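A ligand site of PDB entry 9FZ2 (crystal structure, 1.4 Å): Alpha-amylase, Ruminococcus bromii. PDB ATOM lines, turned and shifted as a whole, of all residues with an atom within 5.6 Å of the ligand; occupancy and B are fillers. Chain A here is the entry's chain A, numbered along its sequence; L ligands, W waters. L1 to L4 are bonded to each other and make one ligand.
The side-chain carboxylate (OD2) of Asp 226 is covalently linked to a carbon (C1) of LIG L1. OD1 of Asp 332 lies within hydrogen-bond range of O4 of LIG L1, at 2.6 Å. The side-chain carboxylate (OD2) of Asp 380 lies within hydrogen-bond range of an oxygen (O2) of LG2 L2 (2.6 Å). NE2 of His 331 lies within hydrogen-bond range of O3 of LIG L1 (2.9 Å). A ring nitrogen (NE2) of His 94 is in hydrogen-bond range of an oxygen (O1) of LG3 L3, 2.9 Å away. A ring nitrogen (NE2) of His 136 lies within hydrogen-bond range of an oxygen (O5) of LIG L1, at 3.0 Å. The guanidinium group (NH2) of Arg 384 sits at hydrogen-bond distance from an oxygen (O1) of LG2 L2. An oxygen (O3) of LIG L1 is in hydrogen-bond range of the guanidinium group (NH2) of Arg 224 (3.1 Å). OG of Ser 191 lies within hydrogen-bond range of O4 of LG3 L3. The side-chain sulfur (SD) of Met 194 sits at hydrogen-bond distance from an oxygen (O5) of LIG L1, at 3.2 Å.
The guanidinium group of Arg 224 lies within salt-bridge range of the side-chain carboxylate of Asp 226. NE2 of His 331 sits at hydrogen-bond distance from OD2 of Asp 332 (3.4 Å). OD1 of Asp 332 lies within salt-bridge range of NH2 of Arg 384 (3.1 Å). OD2 of Asp 380 lies within salt-bridge range of NH2 of Arg 384 (3.8 Å). The side-chain hydroxyl (OG) of Ser 92 sits close to a ring nitrogen (ND1) of His 94. The guanidinium group (NH1) of Arg 224 is in salt-bridge range of the side-chain carboxylate (OD1) of Asp 131 (2.9 Å). The backbone NH (N) of Glu 193 sits at hydrogen-bond distance from the side-chain hydroxyl (OG) of Ser 191 (2.9 Å). N of Ala 227 lies within hydrogen-bond range of OE1 of Glu 261, at 2.9 Å.
Merely in contact with the ligand: Tyr 96, Phe 190, Ala 227 and Glu 193. Hydrophobic or aromatic side chains within 4 Å of the ligand: His 94, Tyr 96, His 136, Phe 190, Met 194, Ala 227 and His 331. Within 4 Å of the ligand: His 94, Tyr 96, His 136, Phe 190, Ser 191, Glu 193, Met 194, Arg 224, Asp 226, Ala 227, His 331, Asp 332, Asp 380 and Arg 384. The nearest printed residue that does not touch the ligand is Asp 97 (4.3 Å).
Water W1 bridges O2 of LG3 L3 and OE2 of Glu 193. Water W3 lies within hydrogen-bond range of the side-chain carboxylate (OE2) of Glu 193 (2.7 Å), the side-chain carboxylate (OD2) of Asp 97 (2.7 Å) and an oxygen (O1) of LG3 L3 (2.7 Å). Water W4 lies within hydrogen-bond range of the side-chain hydroxyl of Ser 191 (2.6 Å) and an oxygen (O5) of LG3 L3 (2.7 Å). Water W6 bridges OH of Tyr 93 (2.8 Å) and O2 of LG2 L2 (2.9 Å). Water W2 bridges an oxygen (O2) of LG3 L3 and a ring nitrogen (NE2) of His 94. Water W5 lies within hydrogen-bond range of the side-chain carboxylate (OE1) of Glu 261 (2.8 Å), an oxygen (O2) of LIG L1 (3.0 Å) and the side-chain carboxylate (OD1) of Asp 226 (3.2 Å).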
ATOM      1  N   PHE A  41      23.742   6.109 -19.694  1.00  0.00           N
ATOM      2  CA  PHE A  41      23.203   7.368 -20.150  1.00  0.00           C
ATOM      3  C   PHE A  41      24.392   8.219 -20.599  1.00  0.00           C
ATOM      4  O   PHE A  41      25.097   8.775 -19.745  1.00  0.00           O
ATOM      5  CB  PHE A  41      22.333   7.991 -19.067  1.00  0.00           C
ATOM      6  CG  PHE A  41      21.533   9.182 -19.556  1.00  0.00           C
ATOM      7  CD1 PHE A  41      20.341   9.005 -20.229  1.00  0.00           C
ATOM      8  CD2 PHE A  41      22.032  10.474 -19.402  1.00  0.00           C
ATOM      9  CE1 PHE A  41      19.642  10.112 -20.706  1.00  0.00           C
ATOM     10  CE2 PHE A  41      21.300  11.588 -19.837  1.00  0.00           C
ATOM     11  CZ  PHE A  41      20.117  11.397 -20.493  1.00  0.00           C
ATOM     12  N   SER A  92      18.680  17.545 -28.041  1.00  0.00           N
ATOM     13  CA  SER A  92      18.467  17.406 -26.603  1.00  0.00           C
ATOM     14  C   SER A  92      19.638  16.663 -25.954  1.00  0.00           C
ATOM     15  O   SER A  92      20.492  16.093 -26.624  1.00  0.00           O
ATOM     16  CB  SER A  92      17.188  16.675 -26.353  1.00  0.00           C
ATOM     17  OG  SER A  92      17.286  15.284 -26.684  1.00  0.00           O
ATOM     18  N   TYR A  93      19.729  16.752 -24.618  1.00  0.00           N
ATOM     19  CA  TYR A  93      20.807  16.056 -23.928  1.00  0.00           C
ATOM     20  C   TYR A  93      20.547  14.543 -23.842  1.00  0.00           C
ATOM     21  O   TYR A  93      21.500  13.786 -23.751  1.00  0.00           O
ATOM     22  CB  TYR A  93      21.014  16.666 -22.529  1.00  0.00           C
ATOM     23  CG  TYR A  93      20.042  16.229 -21.451  1.00  0.00           C
ATOM     24  CD1 TYR A  93      18.744  16.739 -21.358  1.00  0.00           C
ATOM     25  CD2 TYR A  93      20.420  15.266 -20.510  1.00  0.00           C
ATOM     26  CE1 TYR A  93      17.855  16.270 -20.397  1.00  0.00           C
ATOM     27  CE2 TYR A  93      19.545  14.823 -19.544  1.00  0.00           C
ATOM     28  CZ  TYR A  93      18.256  15.305 -19.486  1.00  0.00           C
ATOM     29  OH  TYR A  93      17.365  14.856 -18.547  1.00  0.00           O
ATOM     30  N   HIS A  94      19.277  14.120 -23.900  1.00  0.00           N
ATOM     31  CA  HIS A  94      18.892  12.712 -23.818  1.00  0.00           C
ATOM     32  C   HIS A  94      18.819  12.022 -25.195  1.00  0.00           C
ATOM     33  O   HIS A  94      19.078  10.828 -25.317  1.00  0.00           O
ATOM     34  CB  HIS A  94      17.566  12.574 -23.078  1.00  0.00           C
ATOM     35  CG  HIS A  94      16.473  13.337 -23.716  1.00  0.00           C
ATOM     36  ND1 HIS A  94      15.797  12.907 -24.858  1.00  0.00           N
ATOM     37  CD2 HIS A  94      15.955  14.570 -23.412  1.00  0.00           C
ATOM     38  CE1 HIS A  94      14.907  13.848 -25.173  1.00  0.00           C
ATOM     39  NE2 HIS A  94      14.943  14.818 -24.274  1.00  0.00           N
ATOM     40  N   TYR A  96      16.382  11.228 -27.291  1.00  0.00           N
ATOM     41  CA  TYR A  96      15.298  10.365 -27.729  1.00  0.00           C
ATOM     42  C   TYR A  96      14.483  10.962 -28.875  1.00  0.00           C
ATOM     43  O   TYR A  96      13.635  10.272 -29.447  1.00  0.00           O
ATOM     44  CB  TYR A  96      14.417   9.999 -26.530  1.00  0.00           C
ATOM     45  CG  TYR A  96      15.077   8.926 -25.693  1.00  0.00           C
ATOM     46  CD1 TYR A  96      15.083   7.620 -26.122  1.00  0.00           C
ATOM     47  CD2 TYR A  96      15.776   9.219 -24.522  1.00  0.00           C
ATOM     48  CE1 TYR A  96      15.696   6.615 -25.400  1.00  0.00           C
ATOM     49  CE2 TYR A  96      16.454   8.240 -23.823  1.00  0.00           C
ATOM     50  CZ  TYR A  96      16.373   6.925 -24.242  1.00  0.00           C
ATOM     51  OH  TYR A  96      17.028   5.947 -23.572  1.00  0.00           O
ATOM     52  N   ASP A  97      14.742  12.221 -29.227  1.00  0.00           N
ATOM     53  CA  ASP A  97      14.237  12.870 -30.431  1.00  0.00           C
ATOM     54  C   ASP A  97      15.316  12.811 -31.516  1.00  0.00           C
ATOM     55  O   ASP A  97      16.141  13.692 -31.579  1.00  0.00           O
ATOM     56  CB  ASP A  97      13.800  14.314 -30.135  1.00  0.00           C
ATOM     57  CG  ASP A  97      14.742  15.182 -29.288  1.00  0.00           C
ATOM     58  OD1 ASP A  97      15.347  14.616 -28.361  1.00  0.00           O
ATOM     59  OD2 ASP A  97      14.834  16.428 -29.566  1.00  0.00           O
ATOM     60  N   ASP A 131      20.037   2.029 -28.455  1.00  0.00           N
ATOM     61  CA  ASP A 131      18.681   2.555 -28.305  1.00  0.00           C
ATOM     62  C   ASP A 131      18.180   2.974 -29.683  1.00  0.00           C
ATOM     63  O   ASP A 131      18.540   4.022 -30.214  1.00  0.00           O
ATOM     64  CB  ASP A 131      18.698   3.754 -27.356  1.00  0.00           C
ATOM     65  CG  ASP A 131      17.596   3.727 -26.312  1.00  0.00           C
ATOM     66  OD1 ASP A 131      16.425   3.453 -26.658  1.00  0.00           O
ATOM     67  OD2 ASP A 131      17.915   4.024 -25.102  1.00  0.00           O
ATOM     68  N   HIS A 136       8.932   6.900 -32.619  1.00  0.00           N
ATOM     69  CA  HIS A 136       8.890   8.320 -32.922  1.00  0.00           C
ATOM     70  C   HIS A 136      10.252   8.812 -33.402  1.00  0.00           C
ATOM     71  O   HIS A 136      11.260   8.158 -33.148  1.00  0.00           O
ATOM     72  CB  HIS A 136       8.405   9.144 -31.718  1.00  0.00           C
ATOM     73  CG  HIS A 136       9.070   8.858 -30.416  1.00  0.00           C
ATOM     74  ND1 HIS A 136       8.627   7.845 -29.583  1.00  0.00           N
ATOM     75  CD2 HIS A 136      10.133   9.453 -29.805  1.00  0.00           C
ATOM     76  CE1 HIS A 136       9.351   7.895 -28.490  1.00  0.00           C
ATOM     77  NE2 HIS A 136      10.296   8.815 -28.625  1.00  0.00           N
ATOM     78  N   PHE A 190       4.441  11.662 -26.712  1.00  0.00           N
ATOM     79  CA  PHE A 190       5.469  12.018 -25.739  1.00  0.00           C
ATOM     80  C   PHE A 190       5.814  13.495 -25.727  1.00  0.00           C
ATOM     81  O   PHE A 190       6.151  14.027 -24.647  1.00  0.00           O
ATOM     82  CB  PHE A 190       6.752  11.243 -25.969  1.00  0.00           C
ATOM     83  CG  PHE A 190       6.599   9.777 -25.626  1.00  0.00           C
ATOM     84  CD1 PHE A 190       6.708   9.341 -24.311  1.00  0.00           C
ATOM     85  CD2 PHE A 190       6.429   8.824 -26.631  1.00  0.00           C
ATOM     86  CE1 PHE A 190       6.605   8.011 -23.996  1.00  0.00           C
ATOM     87  CE2 PHE A 190       6.272   7.489 -26.297  1.00  0.00           C
ATOM     88  CZ  PHE A 190       6.383   7.082 -24.987  1.00  0.00           C
ATOM     89  N   SER A 191       5.744  14.139 -26.893  1.00  0.00           N
ATOM     90  CA  SER A 191       6.123  15.526 -27.045  1.00  0.00           C
ATOM     91  C   SER A 191       5.782  16.031 -28.450  1.00  0.00           C
ATOM     92  O   SER A 191       5.851  15.279 -29.416  1.00  0.00           O
ATOM     93  CB  SER A 191       7.608  15.646 -26.826  1.00  0.00           C
ATOM     94  OG  SER A 191       8.164  16.867 -27.266  1.00  0.00           O
ATOM     95  N   GLU A 193       7.850  17.528 -30.069  1.00  0.00           N
ATOM     96  CA  GLU A 193       9.093  17.385 -30.797  1.00  0.00           C
ATOM     97  C   GLU A 193       9.345  15.918 -31.174  1.00  0.00           C
ATOM     98  O   GLU A 193      10.409  15.631 -31.697  1.00  0.00           O
ATOM     99  CB  GLU A 193      10.194  17.964 -29.932  1.00  0.00           C
ATOM    100  CG  GLU A 193      10.108  19.482 -29.872  1.00  0.00           C
ATOM    101  CD  GLU A 193      11.149  20.167 -29.019  1.00  0.00           C
ATOM    102  OE1 GLU A 193      11.215  21.437 -29.148  1.00  0.00           O
ATOM    103  OE2 GLU A 193      11.830  19.502 -28.229  1.00  0.00           O
ATOM    104  N   MET A 194       8.372  15.027 -30.927  1.00  0.00           N
ATOM    105  CA  MET A 194       8.527  13.590 -31.146  1.00  0.00           C
ATOM    106  C   MET A 194       7.333  13.017 -31.914  1.00  0.00           C
ATOM    107  O   MET A 194       6.602  12.170 -31.428  1.00  0.00           O
ATOM    108  CB  MET A 194       8.724  12.869 -29.804  1.00  0.00           C
ATOM    109  CG  MET A 194      10.040  13.192 -29.166  1.00  0.00           C
ATOM    110  SD  MET A 194      10.107  12.780 -27.404  1.00  0.00           S
ATOM    111  CE  MET A 194      11.767  13.305 -26.961  1.00  0.00           C
ATOM    112  N   ARG A 224      17.916  -1.890 -27.867  1.00  0.00           N
ATOM    113  CA  ARG A 224      16.851  -1.626 -26.908  1.00  0.00           C
ATOM    114  C   ARG A 224      15.744  -0.856 -27.639  1.00  0.00           C
ATOM    115  O   ARG A 224      16.024   0.139 -28.316  1.00  0.00           O
ATOM    116  CB  ARG A 224      17.391  -0.861 -25.687  1.00  0.00           C
ATOM    117  CG  ARG A 224      16.290  -0.512 -24.689  1.00  0.00           C
ATOM    118  CD  ARG A 224      15.699   0.873 -24.866  1.00  0.00           C
ATOM    119  NE  ARG A 224      14.917   1.253 -23.695  1.00  0.00           N
ATOM    120  CZ  ARG A 224      14.544   2.504 -23.412  1.00  0.00           C
ATOM    121  NH1 ARG A 224      14.854   3.500 -24.206  1.00  0.00           N
ATOM    122  NH2 ARG A 224      13.877   2.769 -22.300  1.00  0.00           N
ATOM    123  N   ASP A 226      12.529   1.312 -27.236  1.00  0.00           N
ATOM    124  CA  ASP A 226      11.720   2.122 -26.354  1.00  0.00           C
ATOM    125  C   ASP A 226      10.252   2.168 -26.819  1.00  0.00           C
ATOM    126  O   ASP A 226       9.974   2.033 -28.023  1.00  0.00           O
ATOM    127  CB  ASP A 226      12.251   3.540 -26.265  1.00  0.00           C
ATOM    128  CG  ASP A 226      11.882   4.167 -24.947  1.00  0.00           C
ATOM    129  OD1 ASP A 226      11.307   3.646 -24.025  1.00  0.00           O
ATOM    130  OD2 ASP A 226      12.249   5.444 -24.990  1.00  0.00           O
ATOM    131  N   ALA A 227       9.320   2.394 -25.895  1.00  0.00           N
ATOM    132  CA  ALA A 227       7.948   2.824 -26.207  1.00  0.00           C
ATOM    133  C   ALA A 227       7.178   1.771 -26.988  1.00  0.00           C
ATOM    134  O   ALA A 227       6.311   2.111 -27.793  1.00  0.00           O
ATOM    135  CB  ALA A 227       7.977   4.166 -26.951  1.00  0.00           C
ATOM    136  N   GLU A 261      11.197  -2.002 -24.069  1.00  0.00           N
ATOM    137  CA  GLU A 261      10.460  -1.322 -23.024  1.00  0.00           C
ATOM    138  C   GLU A 261       8.969  -1.367 -23.375  1.00  0.00           C
ATOM    139  O   GLU A 261       8.523  -0.670 -24.306  1.00  0.00           O
ATOM    140  CB  GLU A 261      10.810   0.151 -22.929  1.00  0.00           C
ATOM    141  CG  GLU A 261      10.167   0.865 -21.757  1.00  0.00           C
ATOM    142  CD  GLU A 261       9.671   2.265 -22.008  1.00  0.00           C
ATOM    143  OE1 GLU A 261       8.973   2.409 -23.023  1.00  0.00           O
ATOM    144  OE2 GLU A 261       9.823   3.159 -21.188  1.00  0.00           O
ATOM    145  N   HIS A 331      16.794   5.056 -16.311  1.00  0.00           N
ATOM    146  CA  HIS A 331      17.028   6.479 -16.447  1.00  0.00           C
ATOM    147  C   HIS A 331      15.723   7.273 -16.408  1.00  0.00           C
ATOM    148  O   HIS A 331      15.744   8.495 -16.509  1.00  0.00           O
ATOM    149  CB  HIS A 331      17.792   6.771 -17.745  1.00  0.00           C
ATOM    150  CG  HIS A 331      16.979   6.407 -18.948  1.00  0.00           C
ATOM    151  ND1 HIS A 331      16.801   5.123 -19.387  1.00  0.00           N
ATOM    152  CD2 HIS A 331      16.295   7.237 -19.790  1.00  0.00           C
ATOM    153  CE1 HIS A 331      16.085   5.182 -20.516  1.00  0.00           C
ATOM    154  NE2 HIS A 331      15.723   6.462 -20.747  1.00  0.00           N
ATOM    155  N   ASP A 332      14.598   6.563 -16.443  1.00  0.00           N
ATOM    156  CA  ASP A 332      13.283   7.178 -16.365  1.00  0.00           C
ATOM    157  C   ASP A 332      12.648   7.066 -14.981  1.00  0.00           C
ATOM    158  O   ASP A 332      11.475   7.417 -14.821  1.00  0.00           O
ATOM    159  CB  ASP A 332      12.397   6.509 -17.406  1.00  0.00           C
ATOM    160  CG  ASP A 332      12.715   6.841 -18.840  1.00  0.00           C
ATOM    161  OD1 ASP A 332      13.080   8.012 -19.096  1.00  0.00           O
ATOM    162  OD2 ASP A 332      12.482   5.959 -19.698  1.00  0.00           O
ATOM    163  N   ASP A 380      13.411  14.331 -13.992  1.00  0.00           N
ATOM    164  CA  ASP A 380      14.113  13.268 -14.705  1.00  0.00           C
ATOM    165  C   ASP A 380      15.627  13.489 -14.760  1.00  0.00           C
ATOM    166  O   ASP A 380      16.396  12.519 -14.803  1.00  0.00           O
ATOM    167  CB  ASP A 380      13.724  13.230 -16.183  1.00  0.00           C
ATOM    168  CG  ASP A 380      12.383  12.608 -16.525  1.00  0.00           C
ATOM    169  OD1 ASP A 380      11.716  12.069 -15.610  1.00  0.00           O
ATOM    170  OD2 ASP A 380      12.059  12.586 -17.715  1.00  0.00           O
ATOM    171  N   ARG A 384      19.785  11.113 -13.794  1.00  0.00           N
ATOM    172  CA  ARG A 384      20.884  10.966 -14.744  1.00  0.00           C
ATOM    173  C   ARG A 384      22.113  11.768 -14.309  1.00  0.00           C
ATOM    174  O   ARG A 384      22.686  12.491 -15.125  1.00  0.00           O
ATOM    175  CB  ARG A 384      20.365  11.489 -16.078  1.00  0.00           C
ATOM    176  CG  ARG A 384      19.199  10.680 -16.612  1.00  0.00           C
ATOM    177  CD  ARG A 384      18.122  11.583 -17.305  1.00  0.00           C
ATOM    178  NE  ARG A 384      16.995  10.742 -17.718  1.00  0.00           N
ATOM    179  CZ  ARG A 384      16.040  11.155 -18.510  1.00  0.00           C
ATOM    180  NH1 ARG A 384      16.131  12.295 -19.179  1.00  0.00           N
ATOM    181  NH2 ARG A 384      14.975  10.397 -18.633  1.00  0.00           N
HETATM  182  O1  LIG L   1      11.895  10.374 -22.636  1.00  0.00           O
HETATM  183  O2  LIG L   1       9.840   6.916 -25.434  1.00  0.00           O
HETATM  184  C1  LIG L   1      11.736   6.398 -24.069  1.00  0.00           C
HETATM  185  C2  LIG L   1      12.903   6.818 -23.198  1.00  0.00           C
HETATM  186  O3  LIG L   1      13.421   5.797 -22.343  1.00  0.00           O
HETATM  187  C3  LIG L   1      12.530   8.041 -22.383  1.00  0.00           C
HETATM  188  O4  LIG L   1      13.649   8.491 -21.607  1.00  0.00           O
HETATM  189  C4  LIG L   1      12.055   9.131 -23.347  1.00  0.00           C
HETATM  190  C5  LIG L   1      10.742   8.759 -24.031  1.00  0.00           C
HETATM  191  O5  LIG L   1      11.179  10.102 -26.027  1.00  0.00           O
HETATM  192  C6  LIG L   1      10.250   9.808 -24.980  1.00  0.00           C
HETATM  193  C7  LIG L   1      11.024   7.459 -24.811  1.00  0.00           C
HETATM  194  C1  LG2 L   2      12.523  11.532 -23.042  1.00  0.00           C
HETATM  195  C2  LG2 L   2      13.414  12.123 -21.996  1.00  0.00           C
HETATM  196  C3  LG2 L   2      12.534  12.687 -20.949  1.00  0.00           C
HETATM  197  C4  LG2 L   2      11.567  13.709 -21.564  1.00  0.00           C
HETATM  198  C5  LG2 L   2      10.851  13.141 -22.785  1.00  0.00           C
HETATM  199  C6  LG2 L   2      10.200  14.236 -23.566  1.00  0.00           C
HETATM  200  O1  LG2 L   2      14.348  11.151 -21.514  1.00  0.00           O
HETATM  201  O2  LG2 L   2      13.344  13.287 -19.905  1.00  0.00           O
HETATM  202  O3  LG2 L   2      10.522  14.125 -20.680  1.00  0.00           O
HETATM  203  O4  LG2 L   2      11.791  12.519 -23.668  1.00  0.00           O
HETATM  204  O5  LG2 L   2      11.132  15.229 -23.924  1.00  0.00           O
HETATM  205  C1  LG3 L   3      10.636  16.183 -24.857  1.00  0.00           C
HETATM  206  C2  LG3 L   3      11.731  17.224 -25.058  1.00  0.00           C
HETATM  207  C3  LG3 L   3      11.885  18.075 -23.781  1.00  0.00           C
HETATM  208  C4  LG3 L   3      10.513  18.634 -23.361  1.00  0.00           C
HETATM  209  C5  LG3 L   3       9.554  17.480 -23.168  1.00  0.00           C
HETATM  210  C6  LG3 L   3       8.161  17.813 -22.632  1.00  0.00           C
HETATM  211  O1  LG3 L   3      12.955  16.606 -25.446  1.00  0.00           O
HETATM  212  O2  LG3 L   3      12.828  19.122 -24.007  1.00  0.00           O
HETATM  213  O3  LG3 L   3      10.648  19.349 -22.111  1.00  0.00           O
HETATM  214  O4  LG3 L   3       9.414  16.822 -24.445  1.00  0.00           O
HETATM  215  O5  LG3 L   3       7.512  18.747 -23.458  1.00  0.00           O
HETATM  216  C1  LG4 L   4       8.421  20.031 -14.554  1.00  0.00           C
HETATM  217  C2  LG4 L   4       8.884  21.403 -14.985  1.00  0.00           C
HETATM  218  C3  LG4 L   4      10.837  15.283 -19.900  1.00  0.00           C
HETATM  219  C4  LG4 L   4       9.171  18.519 -16.505  1.00  0.00           C
HETATM  220  C5  LG4 L   4       8.013  19.125 -15.719  1.00  0.00           C
HETATM  221  C6  LG4 L   4       8.774  17.366 -17.413  1.00  0.00           C
HETATM  222  C7  LG4 L   4       9.912  16.981 -18.356  1.00  0.00           C
HETATM  223  C8  LG4 L   4       9.595  15.860 -19.320  1.00  0.00           C
HETATM  224  N1  LG4 L   4       9.070  22.425 -13.926  1.00  0.00           N
HETATM  225  O   HOH W   1      12.189  20.927 -25.933  1.00  0.00           O
HETATM  226  O   HOH W   2      15.408  18.066 -23.215  1.00  0.00           O
HETATM  227  O   HOH W   3      13.965  18.012 -27.544  1.00  0.00           O
HETATM  228  O   HOH W   4       7.935  19.139 -26.122  1.00  0.00           O
HETATM  229  O   HOH W   5       8.544   5.154 -23.443  1.00  0.00           O
HETATM  230  O   HOH W   6      14.712  15.619 -18.948  1.00  0.00           O
HETATM  231  O   HOH W   7       5.169  18.563 -25.790  1.00  0.00           O
HETATM  232  O   HOH W   8      12.425  18.910 -20.231  1.00  0.00           O
